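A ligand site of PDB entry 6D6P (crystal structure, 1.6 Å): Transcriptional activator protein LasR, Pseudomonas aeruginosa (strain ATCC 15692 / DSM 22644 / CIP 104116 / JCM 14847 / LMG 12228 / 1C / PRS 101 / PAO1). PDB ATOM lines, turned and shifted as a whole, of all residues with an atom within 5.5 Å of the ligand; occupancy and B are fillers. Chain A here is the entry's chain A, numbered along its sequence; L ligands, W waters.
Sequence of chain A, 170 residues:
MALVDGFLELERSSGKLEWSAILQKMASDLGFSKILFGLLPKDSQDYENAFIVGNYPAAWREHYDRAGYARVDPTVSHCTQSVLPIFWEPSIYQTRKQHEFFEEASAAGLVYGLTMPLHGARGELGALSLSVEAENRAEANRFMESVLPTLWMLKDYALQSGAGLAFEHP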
ATOM      1  N   LEU A  36      12.734  33.450 -29.924  1.00  0.00           N
ATOM      2  CA  LEU A  36      13.620  33.809 -31.013  1.00  0.00           C
ATOM      3  C   LEU A  36      13.137  33.177 -32.306  1.00  0.00           C
ATOM      4  O   LEU A  36      12.978  31.951 -32.393  1.00  0.00           O
ATOM      5  CB  LEU A  36      15.055  33.371 -30.711  1.00  0.00           C
ATOM      6  CG  LEU A  36      16.116  34.057 -31.572  1.00  0.00           C
ATOM      7  CD1 LEU A  36      16.267  35.522 -31.187  1.00  0.00           C
ATOM      8  CD2 LEU A  36      17.432  33.321 -31.436  1.00  0.00           C
ATOM      9  N   TYR A  47      25.386  32.479 -41.892  1.00  0.00           N
ATOM     10  CA  TYR A  47      24.308  33.218 -41.230  1.00  0.00           C
ATOM     11  C   TYR A  47      24.208  34.682 -41.655  1.00  0.00           C
ATOM     12  O   TYR A  47      23.424  35.453 -41.102  1.00  0.00           O
ATOM     13  CB  TYR A  47      24.454  33.142 -39.714  1.00  0.00           C
ATOM     14  CG  TYR A  47      23.986  31.844 -39.128  1.00  0.00           C
ATOM     15  CD1 TYR A  47      24.859  30.766 -38.978  1.00  0.00           C
ATOM     16  CD2 TYR A  47      22.666  31.682 -38.711  1.00  0.00           C
ATOM     17  CE1 TYR A  47      24.429  29.571 -38.452  1.00  0.00           C
ATOM     18  CE2 TYR A  47      22.222  30.480 -38.181  1.00  0.00           C
ATOM     19  CZ  TYR A  47      23.109  29.432 -38.046  1.00  0.00           C
ATOM     20  OH  TYR A  47      22.668  28.254 -37.512  1.00  0.00           O
ATOM     21  N   ILE A  52      16.695  37.292 -38.056  1.00  0.00           N
ATOM     22  CA  ILE A  52      16.586  36.821 -36.670  1.00  0.00           C
ATOM     23  C   ILE A  52      15.980  37.920 -35.817  1.00  0.00           C
ATOM     24  O   ILE A  52      16.528  39.016 -35.697  1.00  0.00           O
ATOM     25  CB  ILE A  52      17.942  36.391 -36.080  1.00  0.00           C
ATOM     26  CG1 ILE A  52      18.560  35.275 -36.942  1.00  0.00           C
ATOM     27  CG2 ILE A  52      17.747  35.917 -34.640  1.00  0.00           C
ATOM     28  CD1 ILE A  52      20.016  34.972 -36.649  1.00  0.00           C
ATOM     29  N   TYR A  56      15.181  37.462 -26.885  1.00  0.00           N
ATOM     30  CA  TYR A  56      16.287  36.863 -26.145  1.00  0.00           C
ATOM     31  C   TYR A  56      17.236  37.989 -25.727  1.00  0.00           C
ATOM     32  O   TYR A  56      17.412  38.960 -26.478  1.00  0.00           O
ATOM     33  CB  TYR A  56      17.074  35.869 -27.010  1.00  0.00           C
ATOM     34  CG  TYR A  56      16.532  34.458 -27.084  1.00  0.00           C
ATOM     35  CD1 TYR A  56      15.198  34.164 -26.751  1.00  0.00           C
ATOM     36  CD2 TYR A  56      17.355  33.412 -27.502  1.00  0.00           C
ATOM     37  CE1 TYR A  56      14.721  32.854 -26.812  1.00  0.00           C
ATOM     38  CE2 TYR A  56      16.880  32.108 -27.572  1.00  0.00           C
ATOM     39  CZ  TYR A  56      15.574  31.831 -27.212  1.00  0.00           C
ATOM     40  OH  TYR A  56      15.109  30.532 -27.300  1.00  0.00           O
ATOM     41  N   TRP A  60      23.269  37.128 -24.295  1.00  0.00           N
ATOM     42  CA  TRP A  60      23.182  35.737 -24.708  1.00  0.00           C
ATOM     43  C   TRP A  60      23.293  35.593 -26.231  1.00  0.00           C
ATOM     44  O   TRP A  60      24.017  34.723 -26.725  1.00  0.00           O
ATOM     45  CB  TRP A  60      21.882  35.103 -24.185  1.00  0.00           C
ATOM     46  CG  TRP A  60      21.669  33.686 -24.611  1.00  0.00           C
ATOM     47  CD1 TRP A  60      20.594  33.208 -25.305  1.00  0.00           C
ATOM     48  CD2 TRP A  60      22.529  32.562 -24.385  1.00  0.00           C
ATOM     49  NE1 TRP A  60      20.725  31.854 -25.517  1.00  0.00           N
ATOM     50  CE2 TRP A  60      21.909  31.430 -24.976  1.00  0.00           C
ATOM     51  CE3 TRP A  60      23.771  32.394 -23.738  1.00  0.00           C
ATOM     52  CZ2 TRP A  60      22.490  30.147 -24.940  1.00  0.00           C
ATOM     53  CZ3 TRP A  60      24.350  31.114 -23.724  1.00  0.00           C
ATOM     54  CH2 TRP A  60      23.698  30.008 -24.316  1.00  0.00           C
ATOM     55  N   ARG A  61      22.604  36.465 -26.962  1.00  0.00           N
ATOM     56  CA  ARG A  61      22.715  36.496 -28.426  1.00  0.00           C
ATOM     57  C   ARG A  61      24.176  36.647 -28.873  1.00  0.00           C
ATOM     58  O   ARG A  61      24.652  35.892 -29.704  1.00  0.00           O
ATOM     59  CB  ARG A  61      21.849  37.605 -29.041  1.00  0.00           C
ATOM     60  CG  ARG A  61      20.346  37.370 -28.948  1.00  0.00           C
ATOM     61  CD  ARG A  61      19.822  36.363 -29.968  1.00  0.00           C
ATOM     62  NE  ARG A  61      20.287  36.688 -31.325  1.00  0.00           N
ATOM     63  CZ  ARG A  61      19.779  37.655 -32.097  1.00  0.00           C
ATOM     64  NH1 ARG A  61      18.780  38.414 -31.682  1.00  0.00           N
ATOM     65  NH2 ARG A  61      20.291  37.853 -33.311  1.00  0.00           N
ATOM     66  N   TYR A  64      26.355  33.435 -27.785  1.00  0.00           N
ATOM     67  CA  TYR A  64      26.026  32.303 -28.636  1.00  0.00           C
ATOM     68  C   TYR A  64      26.765  32.406 -29.976  1.00  0.00           C
ATOM     69  O   TYR A  64      27.317  31.425 -30.458  1.00  0.00           O
ATOM     70  CB  TYR A  64      24.501  32.250 -28.849  1.00  0.00           C
ATOM     71  CG  TYR A  64      23.952  31.057 -29.608  1.00  0.00           C
ATOM     72  CD1 TYR A  64      24.095  30.955 -30.983  1.00  0.00           C
ATOM     73  CD2 TYR A  64      23.237  30.050 -28.944  1.00  0.00           C
ATOM     74  CE1 TYR A  64      23.569  29.880 -31.689  1.00  0.00           C
ATOM     75  CE2 TYR A  64      22.688  28.973 -29.644  1.00  0.00           C
ATOM     76  CZ  TYR A  64      22.879  28.888 -31.012  1.00  0.00           C
ATOM     77  OH  TYR A  64      22.366  27.838 -31.725  1.00  0.00           O
ATOM     78  N   ASP A  65      26.763  33.610 -30.543  1.00  0.00           N
ATOM     79  CA  ASP A  65      27.473  33.889 -31.794  1.00  0.00           C
ATOM     80  C   ASP A  65      28.983  33.724 -31.644  1.00  0.00           C
ATOM     81  O   ASP A  65      29.623  33.004 -32.415  1.00  0.00           O
ATOM     82  CB  ASP A  65      27.143  35.293 -32.294  1.00  0.00           C
ATOM     83  CG  ASP A  65      25.729  35.400 -32.841  1.00  0.00           C
ATOM     84  OD1 ASP A  65      25.012  34.380 -32.848  1.00  0.00           O
ATOM     85  OD2 ASP A  65      25.338  36.502 -33.263  1.00  0.00           O
ATOM     86  N   ASP A  73      24.655  23.655 -30.004  1.00  0.00           N
ATOM     87  CA  ASP A  73      23.231  23.639 -29.717  1.00  0.00           C
ATOM     88  C   ASP A  73      22.549  22.502 -30.475  1.00  0.00           C
ATOM     89  O   ASP A  73      22.492  22.528 -31.699  1.00  0.00           O
ATOM     90  CB  ASP A  73      22.673  25.001 -30.162  1.00  0.00           C
ATOM     91  CG  ASP A  73      21.171  25.126 -30.028  1.00  0.00           C
ATOM     92  OD1 ASP A  73      20.462  24.153 -29.673  1.00  0.00           O
ATOM     93  OD2 ASP A  73      20.704  26.254 -30.269  1.00  0.00           O
ATOM     94  N   THR A  75      19.566  21.688 -31.016  1.00  0.00           N
ATOM     95  CA  THR A  75      18.368  22.007 -31.777  1.00  0.00           C
ATOM     96  C   THR A  75      18.671  22.374 -33.242  1.00  0.00           C
ATOM     97  O   THR A  75      17.811  22.210 -34.110  1.00  0.00           O
ATOM     98  CB  THR A  75      17.536  23.133 -31.122  1.00  0.00           C
ATOM     99  OG1 THR A  75      18.236  24.375 -31.219  1.00  0.00           O
ATOM    100  CG2 THR A  75      17.224  22.830 -29.655  1.00  0.00           C
ATOM    101  N   VAL A  76      19.884  22.854 -33.505  1.00  0.00           N
ATOM    102  CA  VAL A  76      20.273  23.269 -34.867  1.00  0.00           C
ATOM    103  C   VAL A  76      20.256  22.082 -35.829  1.00  0.00           C
ATOM    104  O   VAL A  76      19.529  22.101 -36.825  1.00  0.00           O
ATOM    105  CB  VAL A  76      21.633  23.991 -34.900  1.00  0.00           C
ATOM    106  CG1 VAL A  76      21.994  24.403 -36.328  1.00  0.00           C
ATOM    107  CG2 VAL A  76      21.623  25.216 -34.002  1.00  0.00           C
ATOM    108  N   CYS A  79      16.728  20.632 -36.387  1.00  0.00           N
ATOM    109  CA  CYS A  79      15.913  21.374 -37.347  1.00  0.00           C
ATOM    110  C   CYS A  79      16.211  20.993 -38.819  1.00  0.00           C
ATOM    111  O   CYS A  79      15.315  21.078 -39.672  1.00  0.00           O
ATOM    112  CB  CYS A  79      16.051  22.879 -37.140  1.00  0.00           C
ATOM    113  SG  CYS A  79      15.229  23.514 -35.671  1.00  0.00           S
ATOM    114  N   TRP A  88      13.766  21.328 -24.910  1.00  0.00           N
ATOM    115  CA  TRP A  88      15.101  21.597 -24.360  1.00  0.00           C
ATOM    116  C   TRP A  88      15.364  20.709 -23.166  1.00  0.00           C
ATOM    117  O   TRP A  88      14.774  20.885 -22.104  1.00  0.00           O
ATOM    118  CB  TRP A  88      15.241  23.048 -23.925  1.00  0.00           C
ATOM    119  CG  TRP A  88      14.977  24.084 -24.982  1.00  0.00           C
ATOM    120  CD1 TRP A  88      14.803  23.881 -26.329  1.00  0.00           C
ATOM    121  CD2 TRP A  88      14.890  25.490 -24.767  1.00  0.00           C
ATOM    122  NE1 TRP A  88      14.603  25.094 -26.960  1.00  0.00           N
ATOM    123  CE2 TRP A  88      14.666  26.095 -26.032  1.00  0.00           C
ATOM    124  CE3 TRP A  88      15.001  26.306 -23.636  1.00  0.00           C
ATOM    125  CZ2 TRP A  88      14.517  27.482 -26.181  1.00  0.00           C
ATOM    126  CZ3 TRP A  88      14.859  27.683 -23.779  1.00  0.00           C
ATOM    127  CH2 TRP A  88      14.616  28.257 -25.042  1.00  0.00           C
ATOM    128  N   ILE A  92      19.315  15.815 -24.844  1.00  0.00           N
ATOM    129  CA  ILE A  92      19.707  16.195 -26.203  1.00  0.00           C
ATOM    130  C   ILE A  92      21.141  16.722 -26.165  1.00  0.00           C
ATOM    131  O   ILE A  92      21.821  16.798 -27.188  1.00  0.00           O
ATOM    132  CB  ILE A  92      18.720  17.199 -26.866  1.00  0.00           C
ATOM    133  CG1 ILE A  92      18.621  18.504 -26.064  1.00  0.00           C
ATOM    134  CG2 ILE A  92      17.355  16.542 -27.055  1.00  0.00           C
ATOM    135  CD1 ILE A  92      17.574  19.502 -26.539  1.00  0.00           C
ATOM    136  N   PHE A 101      27.062  24.483 -23.046  1.00  0.00           N
ATOM    137  CA  PHE A 101      25.955  25.221 -23.678  1.00  0.00           C
ATOM    138  C   PHE A 101      24.739  25.258 -22.769  1.00  0.00           C
ATOM    139  O   PHE A 101      24.187  26.339 -22.521  1.00  0.00           O
ATOM    140  CB  PHE A 101      25.580  24.612 -25.034  1.00  0.00           C
ATOM    141  CG  PHE A 101      24.263  25.092 -25.575  1.00  0.00           C
ATOM    142  CD1 PHE A 101      24.154  26.368 -26.128  1.00  0.00           C
ATOM    143  CD2 PHE A 101      23.129  24.284 -25.521  1.00  0.00           C
ATOM    144  CE1 PHE A 101      22.939  26.822 -26.620  1.00  0.00           C
ATOM    145  CE2 PHE A 101      21.914  24.739 -26.013  1.00  0.00           C
ATOM    146  CZ  PHE A 101      21.817  26.011 -26.555  1.00  0.00           C
ATOM    147  N   PHE A 102      24.317  24.103 -22.266  1.00  0.00           N
ATOM    148  CA  PHE A 102      23.149  24.068 -21.368  1.00  0.00           C
ATOM    149  C   PHE A 102      23.357  24.830 -20.066  1.00  0.00           C
ATOM    150  O   PHE A 102      22.457  25.517 -19.595  1.00  0.00           O
ATOM    151  CB  PHE A 102      22.657  22.652 -21.130  1.00  0.00           C
ATOM    152  CG  PHE A 102      21.785  22.142 -22.247  1.00  0.00           C
ATOM    153  CD1 PHE A 102      20.443  22.524 -22.331  1.00  0.00           C
ATOM    154  CD2 PHE A 102      22.298  21.302 -23.218  1.00  0.00           C
ATOM    155  CE1 PHE A 102      19.642  22.070 -23.379  1.00  0.00           C
ATOM    156  CE2 PHE A 102      21.510  20.844 -24.255  1.00  0.00           C
ATOM    157  CZ  PHE A 102      20.182  21.228 -24.335  1.00  0.00           C
ATOM    158  N   ALA A 105      23.177  28.572 -21.032  1.00  0.00           N
ATOM    159  CA  ALA A 105      21.777  28.923 -21.310  1.00  0.00           C
ATOM    160  C   ALA A 105      20.977  29.083 -20.009  1.00  0.00           C
ATOM    161  O   ALA A 105      20.249  30.060 -19.853  1.00  0.00           O
ATOM    162  CB  ALA A 105      21.128  27.891 -22.224  1.00  0.00           C
ATOM    163  N   LEU A 110      17.463  30.884 -19.541  1.00  0.00           N
ATOM    164  CA  LEU A 110      16.762  30.093 -20.552  1.00  0.00           C
ATOM    165  C   LEU A 110      16.931  28.598 -20.276  1.00  0.00           C
ATOM    166  O   LEU A 110      17.850  27.956 -20.787  1.00  0.00           O
ATOM    167  CB  LEU A 110      17.269  30.495 -21.938  1.00  0.00           C
ATOM    168  CG  LEU A 110      17.095  31.997 -22.199  1.00  0.00           C
ATOM    169  CD1 LEU A 110      18.338  32.627 -22.816  1.00  0.00           C
ATOM    170  CD2 LEU A 110      15.853  32.287 -23.032  1.00  0.00           C
ATOM    171  N   THR A 115      12.124  24.173 -29.362  1.00  0.00           N
ATOM    172  CA  THR A 115      12.464  24.777 -30.653  1.00  0.00           C
ATOM    173  C   THR A 115      11.608  24.076 -31.706  1.00  0.00           C
ATOM    174  O   THR A 115      11.628  22.842 -31.828  1.00  0.00           O
ATOM    175  CB  THR A 115      13.971  24.615 -30.940  1.00  0.00           C
ATOM    176  OG1 THR A 115      14.725  25.376 -29.984  1.00  0.00           O
ATOM    177  CG2 THR A 115      14.327  25.091 -32.352  1.00  0.00           C
ATOM    178  N   ALA A 127      13.749  28.358 -37.388  1.00  0.00           N
ATOM    179  CA  ALA A 127      13.317  27.839 -36.096  1.00  0.00           C
ATOM    180  C   ALA A 127      12.592  28.924 -35.319  1.00  0.00           C
ATOM    181  O   ALA A 127      12.954  30.105 -35.379  1.00  0.00           O
ATOM    182  CB  ALA A 127      14.523  27.348 -35.309  1.00  0.00           C
ATOM    183  N   SER A 129      12.074  29.423 -31.505  1.00  0.00           N
ATOM    184  CA  SER A 129      12.476  28.935 -30.187  1.00  0.00           C
ATOM    185  C   SER A 129      11.761  29.723 -29.115  1.00  0.00           C
ATOM    186  O   SER A 129      11.667  30.943 -29.192  1.00  0.00           O
ATOM    187  CB  SER A 129      13.986  29.039 -30.027  1.00  0.00           C
ATOM    188  OG  SER A 129      14.646  28.136 -30.906  1.00  0.00           O
HETATM  189  N1  LIG L   1      18.724  28.957 -25.863  1.00  0.00           N
HETATM  190  C1  LIG L   1      18.463  27.598 -26.060  1.00  0.00           C
HETATM  191  C2  LIG L   1      20.233  31.208 -32.544  1.00  0.00           C
HETATM  192  C3  LIG L   1      19.431  30.108 -32.318  1.00  0.00           C
HETATM  193  C4  LIG L   1      18.037  27.100 -27.298  1.00  0.00           C
HETATM  194  C5  LIG L   1      17.780  27.978 -28.485  1.00  0.00           C
HETATM  195  C6  LIG L   1      18.000  24.858 -26.387  1.00  0.00           C
HETATM  196  C7  LIG L   1      18.646  26.718 -24.993  1.00  0.00           C
HETATM  197  C8  LIG L   1      18.031  26.560 -34.120  1.00  0.00           C
HETATM  198  C9  LIG L   1      18.218  28.547 -30.821  1.00  0.00           C
HETATM  199  C10 LIG L   1      19.093  29.757 -31.015  1.00  0.00           C
HETATM  200  C11 LIG L   1      19.538  30.538 -29.945  1.00  0.00           C
HETATM  201  C12 LIG L   1      20.349  31.661 -30.191  1.00  0.00           C
HETATM  202  C13 LIG L   1      20.691  32.000 -31.501  1.00  0.00           C
HETATM  203  O1  LIG L   1      16.912  28.841 -28.386  1.00  0.00           O
HETATM  204  O2  LIG L   1      18.945  27.457 -34.759  1.00  0.00           O
HETATM  205  C14 LIG L   1      19.722  28.206 -33.831  1.00  0.00           C
HETATM  206  O3  LIG L   1      18.987  29.341 -33.367  1.00  0.00           O
HETATM  207 BR1  LIG L   1      20.687  31.641 -34.334  1.00  0.00          BR
HETATM  208 BR2  LIG L   1      20.956  32.722 -28.758  1.00  0.00          BR
HETATM  209  N2  LIG L   1      18.453  27.781 -29.605  1.00  0.00           N
HETATM  210  O4  LIG L   1      18.455  29.504 -24.628  1.00  0.00           O
HETATM  211  O5  LIG L   1      19.230  29.653 -26.739  1.00  0.00           O
HETATM  212  C15 LIG L   1      17.804  25.736 -27.458  1.00  0.00           C
HETATM  213  C16 LIG L   1      18.413  25.354 -25.153  1.00  0.00           C
HETATM  214  O   HOH W   1      19.975  28.388 -37.309  1.00  0.00           O
HETATM  215  O   HOH W   2      16.780  30.273 -35.187  1.00  0.00           O
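The side-chain carboxylate (OD2) of Asp 73 sits at hydrogen-bond distance from a nitrogen (N2) of the ligand (2.8 Å).
O5 of the ligand sits at hydrogen-bond distance from NE1 of Trp 60 (2.9 Å).
The side-chain hydroxyl (OH) of Tyr 56 lies within hydrogen-bond range of an oxygen (O1) of the ligand (2.7 Å).
OG of Ser 129 lies close to O1 of the ligand (3.5 Å).
OD2 of Asp 73 sits at hydrogen-bond distance from OH of Tyr 64 (2.7 Å).
OD1 of Asp 73 sits at hydrogen-bond distance from OG1 of Thr 75, at 2.7 Å.
N of Leu 36 lies within hydrogen-bond range of O of Ser 129 (2.8 Å).
The side-chain hydroxyl (OG1) of Thr 115 is in hydrogen-bond range of the side-chain hydroxyl (OG) of Ser 129 (2.9 Å).
The backbone NH of Leu 110 lies within hydrogen-bond range of the backbone carbonyl oxygen of Ala 105 (2.9 Å).
NE1 of Trp 88 lies within hydrogen-bond range of OG1 of Thr 115 (3.0 Å).
The backbone carbonyl oxygen (O) of Thr 75 is in hydrogen-bond range of the side-chain sulfur (SG) of Cys 79 (3.3 Å).
Leu 36 touches the ligand.
Tyr 64 touches the ligand.
Thr 75 touches the ligand (OG1 to C8, 3.6 Å).
CG2 of Val 76 touches C14 of the ligand (3.5 Å).
Trp 88 touches the ligand.
Phe 101 touches the ligand.
CE1 of Phe 102 touches C16 of the ligand, at 3.9 Å.
Ala 105 touches the ligand (CB to C7, 3.9 Å).
Leu 110 touches the ligand.
Thr 115 touches the ligand.
Ala 127 touches the ligand.
Hydrophobic or aromatic side chains that line the ligand: Leu 36, Tyr 56, Trp 60, Tyr 64, Val 76, Trp 88, Phe 101, Phe 102, Ala 105, Leu 110 and Ala 127.
Within 4 Å of the ligand: Leu 36, Tyr 56, Trp 60, Tyr 64, Asp 73, Thr 75, Val 76, Trp 88, Phe 101, Phe 102, Ala 105, Leu 110, Thr 115, Ala 127 and Ser 129.
The nearest printed residue that does not touch the ligand is Arg 61 (4.001 Å).
Water W1 bridges OH of Tyr 47 (2.7 Å) and O2 of the ligand (2.9 Å).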
